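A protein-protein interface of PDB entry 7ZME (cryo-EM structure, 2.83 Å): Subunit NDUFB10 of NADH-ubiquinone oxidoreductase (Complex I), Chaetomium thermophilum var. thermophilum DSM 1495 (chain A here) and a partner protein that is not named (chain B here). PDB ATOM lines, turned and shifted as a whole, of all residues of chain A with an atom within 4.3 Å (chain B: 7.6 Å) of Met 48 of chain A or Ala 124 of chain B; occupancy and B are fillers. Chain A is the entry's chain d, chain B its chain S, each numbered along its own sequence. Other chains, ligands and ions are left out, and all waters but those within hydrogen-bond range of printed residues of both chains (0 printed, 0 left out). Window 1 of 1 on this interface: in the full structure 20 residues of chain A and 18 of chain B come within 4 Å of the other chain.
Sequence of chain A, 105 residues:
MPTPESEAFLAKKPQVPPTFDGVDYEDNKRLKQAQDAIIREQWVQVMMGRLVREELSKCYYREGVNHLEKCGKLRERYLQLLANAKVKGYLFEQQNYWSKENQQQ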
ATOM      1  N   VAL A  44      20.404  15.302  -3.758  1.00  0.00           N
ATOM      2  CA  VAL A  44      21.617  14.568  -3.410  1.00  0.00           C
ATOM      3  C   VAL A  44      21.462  13.878  -2.060  1.00  0.00           C
ATOM      4  O   VAL A  44      21.846  12.716  -1.895  1.00  0.00           O
ATOM      5  CB  VAL A  44      22.840  15.505  -3.435  1.00  0.00           C
ATOM      6  CG1 VAL A  44      24.025  14.850  -2.752  1.00  0.00           C
ATOM      7  CG2 VAL A  44      23.202  15.848  -4.865  1.00  0.00           C
ATOM      8  N   GLN A  45      20.893  14.577  -1.078  1.00  0.00           N
ATOM      9  CA  GLN A  45      20.699  13.977   0.236  1.00  0.00           C
ATOM     10  C   GLN A  45      19.780  12.770   0.156  1.00  0.00           C
ATOM     11  O   GLN A  45      19.974  11.782   0.870  1.00  0.00           O
ATOM     12  CB  GLN A  45      20.133  15.012   1.205  1.00  0.00           C
ATOM     13  CG  GLN A  45      20.974  16.253   1.331  1.00  0.00           C
ATOM     14  CD  GLN A  45      22.398  15.940   1.715  1.00  0.00           C
ATOM     15  OE1 GLN A  45      23.343  16.429   1.096  1.00  0.00           O
ATOM     16  NE2 GLN A  45      22.565  15.123   2.743  1.00  0.00           N
ATOM     17  N   VAL A  46      18.760  12.844  -0.696  1.00  0.00           N
ATOM     18  CA  VAL A  46      17.842  11.726  -0.858  1.00  0.00           C
ATOM     19  C   VAL A  46      18.522  10.576  -1.584  1.00  0.00           C
ATOM     20  O   VAL A  46      18.337   9.406  -1.228  1.00  0.00           O
ATOM     21  CB  VAL A  46      16.575  12.201  -1.587  1.00  0.00           C
ATOM     22  CG1 VAL A  46      15.722  11.018  -2.013  1.00  0.00           C
ATOM     23  CG2 VAL A  46      15.805  13.150  -0.703  1.00  0.00           C
ATOM     24  N   MET A  47      19.317  10.882  -2.612  1.00  0.00           N
ATOM     25  CA  MET A  47      20.055   9.829  -3.296  1.00  0.00           C
ATOM     26  C   MET A  47      21.175   9.276  -2.428  1.00  0.00           C
ATOM     27  O   MET A  47      21.650   8.166  -2.682  1.00  0.00           O
ATOM     28  CB  MET A  47      20.631  10.337  -4.615  1.00  0.00           C
ATOM     29  CG  MET A  47      19.597  10.731  -5.659  1.00  0.00           C
ATOM     30  SD  MET A  47      18.472   9.457  -6.246  1.00  0.00           S
ATOM     31  CE  MET A  47      16.999   9.892  -5.330  1.00  0.00           C
ATOM     32  N   MET A  48      21.606  10.034  -1.415  1.00  0.00           N
ATOM     33  CA  MET A  48      22.491   9.484  -0.394  1.00  0.00           C
ATOM     34  C   MET A  48      21.789   8.390   0.392  1.00  0.00           C
ATOM     35  O   MET A  48      22.419   7.413   0.812  1.00  0.00           O
ATOM     36  CB  MET A  48      22.962  10.600   0.539  1.00  0.00           C
ATOM     37  CG  MET A  48      24.289  11.226   0.154  1.00  0.00           C
ATOM     38  SD  MET A  48      24.680  12.689   1.117  1.00  0.00           S
ATOM     39  CE  MET A  48      25.716  11.996   2.396  1.00  0.00           C
ATOM     40  N   GLY A  49      20.481   8.540   0.605  1.00  0.00           N
ATOM     41  CA  GLY A  49      19.715   7.475   1.227  1.00  0.00           C
ATOM     42  C   GLY A  49      19.662   6.219   0.378  1.00  0.00           C
ATOM     43  O   GLY A  49      19.810   5.110   0.890  1.00  0.00           O
ATOM     44  N   ARG A  50      19.452   6.377  -0.932  1.00  0.00           N
ATOM     45  CA  ARG A  50      19.359   5.212  -1.806  1.00  0.00           C
ATOM     46  C   ARG A  50      20.662   4.429  -1.839  1.00  0.00           C
ATOM     47  O   ARG A  50      20.646   3.193  -1.846  1.00  0.00           O
ATOM     48  CB  ARG A  50      18.948   5.630  -3.218  1.00  0.00           C
ATOM     49  CG  ARG A  50      17.479   5.985  -3.343  1.00  0.00           C
ATOM     50  CD  ARG A  50      17.135   6.504  -4.724  1.00  0.00           C
ATOM     51  NE  ARG A  50      17.408   5.534  -5.776  1.00  0.00           N
ATOM     52  CZ  ARG A  50      17.282   5.787  -7.073  1.00  0.00           C
ATOM     53  NH1 ARG A  50      17.559   4.850  -7.966  1.00  0.00           N
ATOM     54  NH2 ARG A  50      16.856   6.973  -7.480  1.00  0.00           N
ATOM     55  N   LEU A  51      21.797   5.123  -1.869  1.00  0.00           N
ATOM     56  CA  LEU A  51      23.074   4.424  -1.891  1.00  0.00           C
ATOM     57  C   LEU A  51      23.316   3.686  -0.582  1.00  0.00           C
ATOM     58  O   LEU A  51      23.607   2.490  -0.588  1.00  0.00           O
ATOM     59  CB  LEU A  51      24.204   5.406  -2.178  1.00  0.00           C
ATOM     60  CG  LEU A  51      24.326   5.857  -3.628  1.00  0.00           C
ATOM     61  CD1 LEU A  51      25.378   6.942  -3.755  1.00  0.00           C
ATOM     62  CD2 LEU A  51      24.652   4.674  -4.515  1.00  0.00           C
ATOM     63  N   VAL A  52      23.155   4.377   0.551  1.00  0.00           N
ATOM     64  CA  VAL A  52      23.333   3.747   1.859  1.00  0.00           C
ATOM     65  C   VAL A  52      22.370   2.584   2.022  1.00  0.00           C
ATOM     66  O   VAL A  52      22.724   1.534   2.573  1.00  0.00           O
ATOM     67  CB  VAL A  52      23.152   4.788   2.982  1.00  0.00           C
ATOM     68  CG1 VAL A  52      23.036   4.105   4.336  1.00  0.00           C
ATOM     69  CG2 VAL A  52      24.308   5.770   2.982  1.00  0.00           C
ATOM     70  N   LEU A  81      19.416   9.713   7.358  1.00  0.00           N
ATOM     71  CA  LEU A  81      19.056  10.237   6.048  1.00  0.00           C
ATOM     72  C   LEU A  81      17.560  10.128   5.796  1.00  0.00           C
ATOM     73  O   LEU A  81      16.976  11.009   5.158  1.00  0.00           O
ATOM     74  CB  LEU A  81      19.842   9.507   4.962  1.00  0.00           C
ATOM     75  CG  LEU A  81      21.242  10.063   4.698  1.00  0.00           C
ATOM     76  CD1 LEU A  81      22.138   9.020   4.059  1.00  0.00           C
ATOM     77  CD2 LEU A  81      21.167  11.309   3.837  1.00  0.00           C
ATOM     78  N   GLN B 117      18.487  12.015 -10.917  1.00  0.00           N
ATOM     79  CA  GLN B 117      19.077  10.966 -10.091  1.00  0.00           C
ATOM     80  C   GLN B 117      20.525  10.696 -10.475  1.00  0.00           C
ATOM     81  O   GLN B 117      21.429  10.825  -9.646  1.00  0.00           O
ATOM     82  CB  GLN B 117      18.248   9.685 -10.184  1.00  0.00           C
ATOM     83  CG  GLN B 117      16.885   9.817  -9.567  1.00  0.00           C
ATOM     84  CD  GLN B 117      15.891  10.472 -10.476  1.00  0.00           C
ATOM     85  OE1 GLN B 117      16.089  10.562 -11.688  1.00  0.00           O
ATOM     86  NE2 GLN B 117      14.825  10.982  -9.887  1.00  0.00           N
ATOM     87  N   TRP B 119      22.582  12.381 -11.934  1.00  0.00           N
ATOM     88  CA  TRP B 119      23.416  13.499 -11.510  1.00  0.00           C
ATOM     89  C   TRP B 119      23.634  13.475 -10.004  1.00  0.00           C
ATOM     90  O   TRP B 119      24.746  13.713  -9.525  1.00  0.00           O
ATOM     91  CB  TRP B 119      22.790  14.826 -11.934  1.00  0.00           C
ATOM     92  CG  TRP B 119      23.636  16.012 -11.585  1.00  0.00           C
ATOM     93  CD1 TRP B 119      24.558  16.621 -12.381  1.00  0.00           C
ATOM     94  CD2 TRP B 119      23.649  16.727 -10.342  1.00  0.00           C
ATOM     95  NE1 TRP B 119      25.143  17.668 -11.715  1.00  0.00           N
ATOM     96  CE2 TRP B 119      24.603  17.753 -10.460  1.00  0.00           C
ATOM     97  CE3 TRP B 119      22.950  16.594  -9.139  1.00  0.00           C
ATOM     98  CZ2 TRP B 119      24.869  18.642  -9.429  1.00  0.00           C
ATOM     99  CZ3 TRP B 119      23.219  17.473  -8.118  1.00  0.00           C
ATOM    100  CH2 TRP B 119      24.168  18.486  -8.267  1.00  0.00           C
ATOM    101  N   ALA B 120      22.576  13.204  -9.242  1.00  0.00           N
ATOM    102  CA  ALA B 120      22.679  13.220  -7.791  1.00  0.00           C
ATOM    103  C   ALA B 120      23.350  11.966  -7.245  1.00  0.00           C
ATOM    104  O   ALA B 120      23.991  12.031  -6.193  1.00  0.00           O
ATOM    105  CB  ALA B 120      21.295  13.406  -7.172  1.00  0.00           C
ATOM    106  N   LEU B 121      23.214  10.824  -7.925  1.00  0.00           N
ATOM    107  CA  LEU B 121      23.976   9.644  -7.521  1.00  0.00           C
ATOM    108  C   LEU B 121      25.472   9.904  -7.590  1.00  0.00           C
ATOM    109  O   LEU B 121      26.231   9.408  -6.752  1.00  0.00           O
ATOM    110  CB  LEU B 121      23.615   8.426  -8.377  1.00  0.00           C
ATOM    111  CG  LEU B 121      22.400   7.540  -8.073  1.00  0.00           C
ATOM    112  CD1 LEU B 121      22.574   6.861  -6.724  1.00  0.00           C
ATOM    113  CD2 LEU B 121      21.087   8.259  -8.116  1.00  0.00           C
ATOM    114  N   GLU B 122      25.917  10.667  -8.588  1.00  0.00           N
ATOM    115  CA  GLU B 122      27.342  10.953  -8.715  1.00  0.00           C
ATOM    116  C   GLU B 122      27.845  11.766  -7.531  1.00  0.00           C
ATOM    117  O   GLU B 122      28.851  11.412  -6.909  1.00  0.00           O
ATOM    118  CB  GLU B 122      27.617  11.670 -10.034  1.00  0.00           C
ATOM    119  CG  GLU B 122      27.371  10.797 -11.254  1.00  0.00           C
ATOM    120  CD  GLU B 122      27.626  11.515 -12.563  1.00  0.00           C
ATOM    121  OE1 GLU B 122      27.878  12.736 -12.536  1.00  0.00           O
ATOM    122  OE2 GLU B 122      27.568  10.856 -13.624  1.00  0.00           O
ATOM    123  N   GLU B 123      27.153  12.857  -7.197  1.00  0.00           N
ATOM    124  CA  GLU B 123      27.557  13.650  -6.042  1.00  0.00           C
ATOM    125  C   GLU B 123      27.418  12.856  -4.753  1.00  0.00           C
ATOM    126  O   GLU B 123      28.355  12.808  -3.949  1.00  0.00           O
ATOM    127  CB  GLU B 123      26.737  14.935  -5.962  1.00  0.00           C
ATOM    128  CG  GLU B 123      27.171  15.875  -4.845  1.00  0.00           C
ATOM    129  CD  GLU B 123      28.655  16.201  -4.887  1.00  0.00           C
ATOM    130  OE1 GLU B 123      29.284  16.247  -3.809  1.00  0.00           O
ATOM    131  OE2 GLU B 123      29.195  16.418  -5.994  1.00  0.00           O
ATOM    132  N   ALA B 124      26.263  12.220  -4.548  1.00  0.00           N
ATOM    133  CA  ALA B 124      26.046  11.443  -3.334  1.00  0.00           C
ATOM    134  C   ALA B 124      27.079  10.337  -3.185  1.00  0.00           C
ATOM    135  O   ALA B 124      27.440   9.974  -2.060  1.00  0.00           O
ATOM    136  CB  ALA B 124      24.636  10.854  -3.332  1.00  0.00           C
ATOM    137  N   ARG B 125      27.559   9.789  -4.301  1.00  0.00           N
ATOM    138  CA  ARG B 125      28.626   8.800  -4.231  1.00  0.00           C
ATOM    139  C   ARG B 125      29.882   9.407  -3.622  1.00  0.00           C
ATOM    140  O   ARG B 125      30.530   8.790  -2.770  1.00  0.00           O
ATOM    141  CB  ARG B 125      28.913   8.245  -5.624  1.00  0.00           C
ATOM    142  CG  ARG B 125      30.029   7.220  -5.677  1.00  0.00           C
ATOM    143  CD  ARG B 125      29.741   6.046  -4.748  1.00  0.00           C
ATOM    144  NE  ARG B 125      28.699   5.130  -5.222  1.00  0.00           N
ATOM    145  CZ  ARG B 125      28.640   4.565  -6.428  1.00  0.00           C
ATOM    146  NH1 ARG B 125      27.629   3.758  -6.717  1.00  0.00           N
ATOM    147  NH2 ARG B 125      29.591   4.761  -7.333  1.00  0.00           N
ATOM    148  N   ARG B 126      30.230  10.625  -4.037  1.00  0.00           N
ATOM    149  CA  ARG B 126      31.378  11.314  -3.460  1.00  0.00           C
ATOM    150  C   ARG B 126      31.140  11.672  -1.998  1.00  0.00           C
ATOM    151  O   ARG B 126      32.059  11.577  -1.177  1.00  0.00           O
ATOM    152  CB  ARG B 126      31.692  12.567  -4.271  1.00  0.00           C
ATOM    153  CG  ARG B 126      32.299  12.280  -5.627  1.00  0.00           C
ATOM    154  CD  ARG B 126      32.554  13.565  -6.383  1.00  0.00           C
ATOM    155  NE  ARG B 126      31.325  14.100  -6.957  1.00  0.00           N
ATOM    156  CZ  ARG B 126      30.887  13.818  -8.178  1.00  0.00           C
ATOM    157  NH1 ARG B 126      29.762  14.352  -8.615  1.00  0.00           N
ATOM    158  NH2 ARG B 126      31.579  13.008  -8.963  1.00  0.00           N
ATOM    159  N   ARG B 127      29.924  12.099  -1.656  1.00  0.00           N
ATOM    160  CA  ARG B 127      29.646  12.492  -0.277  1.00  0.00           C
ATOM    161  C   ARG B 127      29.755  11.306   0.669  1.00  0.00           C
ATOM    162  O   ARG B 127      30.254  11.444   1.790  1.00  0.00           O
ATOM    163  CB  ARG B 127      28.265  13.133  -0.174  1.00  0.00           C
ATOM    164  CG  ARG B 127      28.004  14.197  -1.209  1.00  0.00           C
ATOM    165  CD  ARG B 127      28.177  15.581  -0.632  1.00  0.00           C
ATOM    166  NE  ARG B 127      27.698  16.604  -1.553  1.00  0.00           N
ATOM    167  CZ  ARG B 127      26.628  17.357  -1.336  1.00  0.00           C
ATOM    168  NH1 ARG B 127      25.932  17.209  -0.221  1.00  0.00           N
ATOM    169  NH2 ARG B 127      26.262  18.263  -2.228  1.00  0.00           N
ATOM    170  N   LEU B 128      29.283  10.137   0.243  1.00  0.00           N
ATOM    171  CA  LEU B 128      29.441   8.945   1.067  1.00  0.00           C
ATOM    172  C   LEU B 128      30.860   8.403   0.987  1.00  0.00           C
ATOM    173  O   LEU B 128      31.316   7.730   1.918  1.00  0.00           O
ATOM    174  CB  LEU B 128      28.430   7.883   0.645  1.00  0.00           C
ATOM    175  CG  LEU B 128      26.975   8.320   0.814  1.00  0.00           C
ATOM    176  CD1 LEU B 128      26.039   7.323   0.181  1.00  0.00           C
ATOM    177  CD2 LEU B 128      26.646   8.506   2.277  1.00  0.00           C
ATOM    178  N   GLU B 129      31.569   8.684  -0.109  1.00  0.00           N
ATOM    179  CA  GLU B 129      32.974   8.304  -0.204  1.00  0.00           C
ATOM    180  C   GLU B 129      33.814   9.019   0.842  1.00  0.00           C
ATOM    181  O   GLU B 129      34.762   8.436   1.379  1.00  0.00           O
ATOM    182  CB  GLU B 129      33.512   8.600  -1.603  1.00  0.00           C
ATOM    183  CG  GLU B 129      33.368   7.450  -2.583  1.00  0.00           C
ATOM    184  CD  GLU B 129      33.522   7.891  -4.024  1.00  0.00           C
ATOM    185  OE1 GLU B 129      33.210   7.090  -4.929  1.00  0.00           O
ATOM    186  OE2 GLU B 129      33.959   9.039  -4.252  1.00  0.00           O
ATOM    187  N   ALA B 130      33.490  10.276   1.143  1.00  0.00           N
ATOM    188  CA  ALA B 130      34.188  10.994   2.199  1.00  0.00           C
ATOM    189  C   ALA B 130      33.586  10.654   3.555  1.00  0.00           C
ATOM    190  O   ALA B 130      33.300  11.545   4.359  1.00  0.00           O
ATOM    191  CB  ALA B 130      34.133  12.501   1.950  1.00  0.00           C
ATOM    192  N   GLU B 131      33.431   9.364   3.819  1.00  0.00           N
ATOM    193  CA  GLU B 131      32.879   8.808   5.052  1.00  0.00           C
ATOM    194  C   GLU B 131      33.408   7.383   5.164  1.00  0.00           C
ATOM    195  O   GLU B 131      34.308   6.981   4.416  1.00  0.00           O
ATOM    196  CB  GLU B 131      31.347   8.841   5.063  1.00  0.00           C
ATOM    197  CG  GLU B 131      30.716  10.219   5.192  1.00  0.00           C
ATOM    198  CD  GLU B 131      29.205  10.181   5.085  1.00  0.00           C
ATOM    199  OE1 GLU B 131      28.657   9.099   4.796  1.00  0.00           O
ATOM    200  OE2 GLU B 131      28.565  11.235   5.287  1.00  0.00           O
ATOM    201  N   ILE B 133      31.725   4.815   4.371  1.00  0.00           N
ATOM    202  CA  ILE B 133      30.976   4.019   3.405  1.00  0.00           C
ATOM    203  C   ILE B 133      31.640   4.158   2.042  1.00  0.00           C
ATOM    204  O   ILE B 133      32.297   5.163   1.755  1.00  0.00           O
ATOM    205  CB  ILE B 133      29.497   4.468   3.367  1.00  0.00           C
ATOM    206  CG1 ILE B 133      28.853   4.358   4.751  1.00  0.00           C
ATOM    207  CG2 ILE B 133      28.690   3.639   2.383  1.00  0.00           C
ATOM    208  CD1 ILE B 133      28.935   5.626   5.574  1.00  0.00           C
ATOM    209  N   LEU B 134      31.481   3.138   1.195  1.00  0.00           N
ATOM    210  CA  LEU B 134      31.811   3.227  -0.226  1.00  0.00           C
ATOM    211  C   LEU B 134      33.289   3.572  -0.437  1.00  0.00           C
ATOM    212  O   LEU B 134      33.649   4.671  -0.862  1.00  0.00           O
ATOM    213  CB  LEU B 134      30.903   4.247  -0.922  1.00  0.00           C
ATOM    214  CG  LEU B 134      29.570   3.706  -1.433  1.00  0.00           C
ATOM    215  CD1 LEU B 134      28.559   4.828  -1.593  1.00  0.00           C
ATOM    216  CD2 LEU B 134      29.767   2.962  -2.747  1.00  0.00           C
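The side-chain amide oxygen (OE1) of Gln 45 of chain A sits at hydrogen-bond distance from the guanidinium group (NH1) of Arg 127 of chain B (3.0 Å).
OE2 of Glu 123 of chain B is in salt-bridge range of NE of Arg 126 of chain B (3.3 Å). NE of Arg 127 of chain B is in salt-bridge range of OE1 of Glu 123 of chain B, at 2.8 Å. SD of Met 48 of chain A lies within hydrogen-bond range of NE2 of Gln 45 of chain A (3.6 Å). NH2 of Arg 50 of chain A sits at hydrogen-bond distance from SD of Met 47 of chain A, 3.2 Å away.
CG2 of Val 44 of chain A touches CZ3 of Trp 119 of chain B, at 3.6 Å. CB of Ala 120 of chain B touches CG2 of Val 44 of chain A, 3.9 Å away. Glu 123 of chain B touches Val 44 of chain A. Arg 127 of chain B touches Val 44 of chain A (CZ to CG1, 3.9 Å). Ala 120 of chain B touches Met 47 of chain A. Met 47 of chain A touches Ala 124 of chain B. CB of Arg 127 of chain B touches CE of Met 48 of chain A, 3.8 Å away. CD2 of Leu 128 of chain B touches CE of Met 48 of chain A, at 3.6 Å. Leu 51 of chain A touches Leu 121 of chain B (CG to CD1, 3.7 Å). CD1 of Leu 51 of chain A touches N of Arg 125 of chain B (3.6 Å).
Met 48 of chain A touches just these residues of chain B: Ala 124 (3.5 Å), Arg 127 (3.8 Å) and Leu 128 (3.6 Å). Of the printed residues of chain A, Ala 120 of chain B touches Val 44 and Met 47. Printed residues of chain A within 4 Å of Leu 121 of chain B: Met 47 and Leu 51. Of the printed residues of chain A, Glu 123 of chain B touches Val 44. Of the printed residues of chain A, Arg 125 of chain B touches Leu 51 (3.6 Å). The nearest printed residue of chain A that does not touch Ala 124 of chain B is Gln 45 of chain A (5.7 Å). The nearest printed residue of chain A that does not touch Leu 128 of chain B is Leu 81 of chain A (4.9 Å).
Printed residues of chain A that touch a printed residue of chain B: Val 44, Gln 45, Met 47, Met 48, Arg 50, Leu 51 and Val 52. Of the 16 printed residues of chain B, 9 touch a printed residue of chain A. Hydrophobic or aromatic side chains of chain B within 4 Å of the printed part of chain A: Trp 119, Ala 120, Leu 121, Ala 124 and Leu 128.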
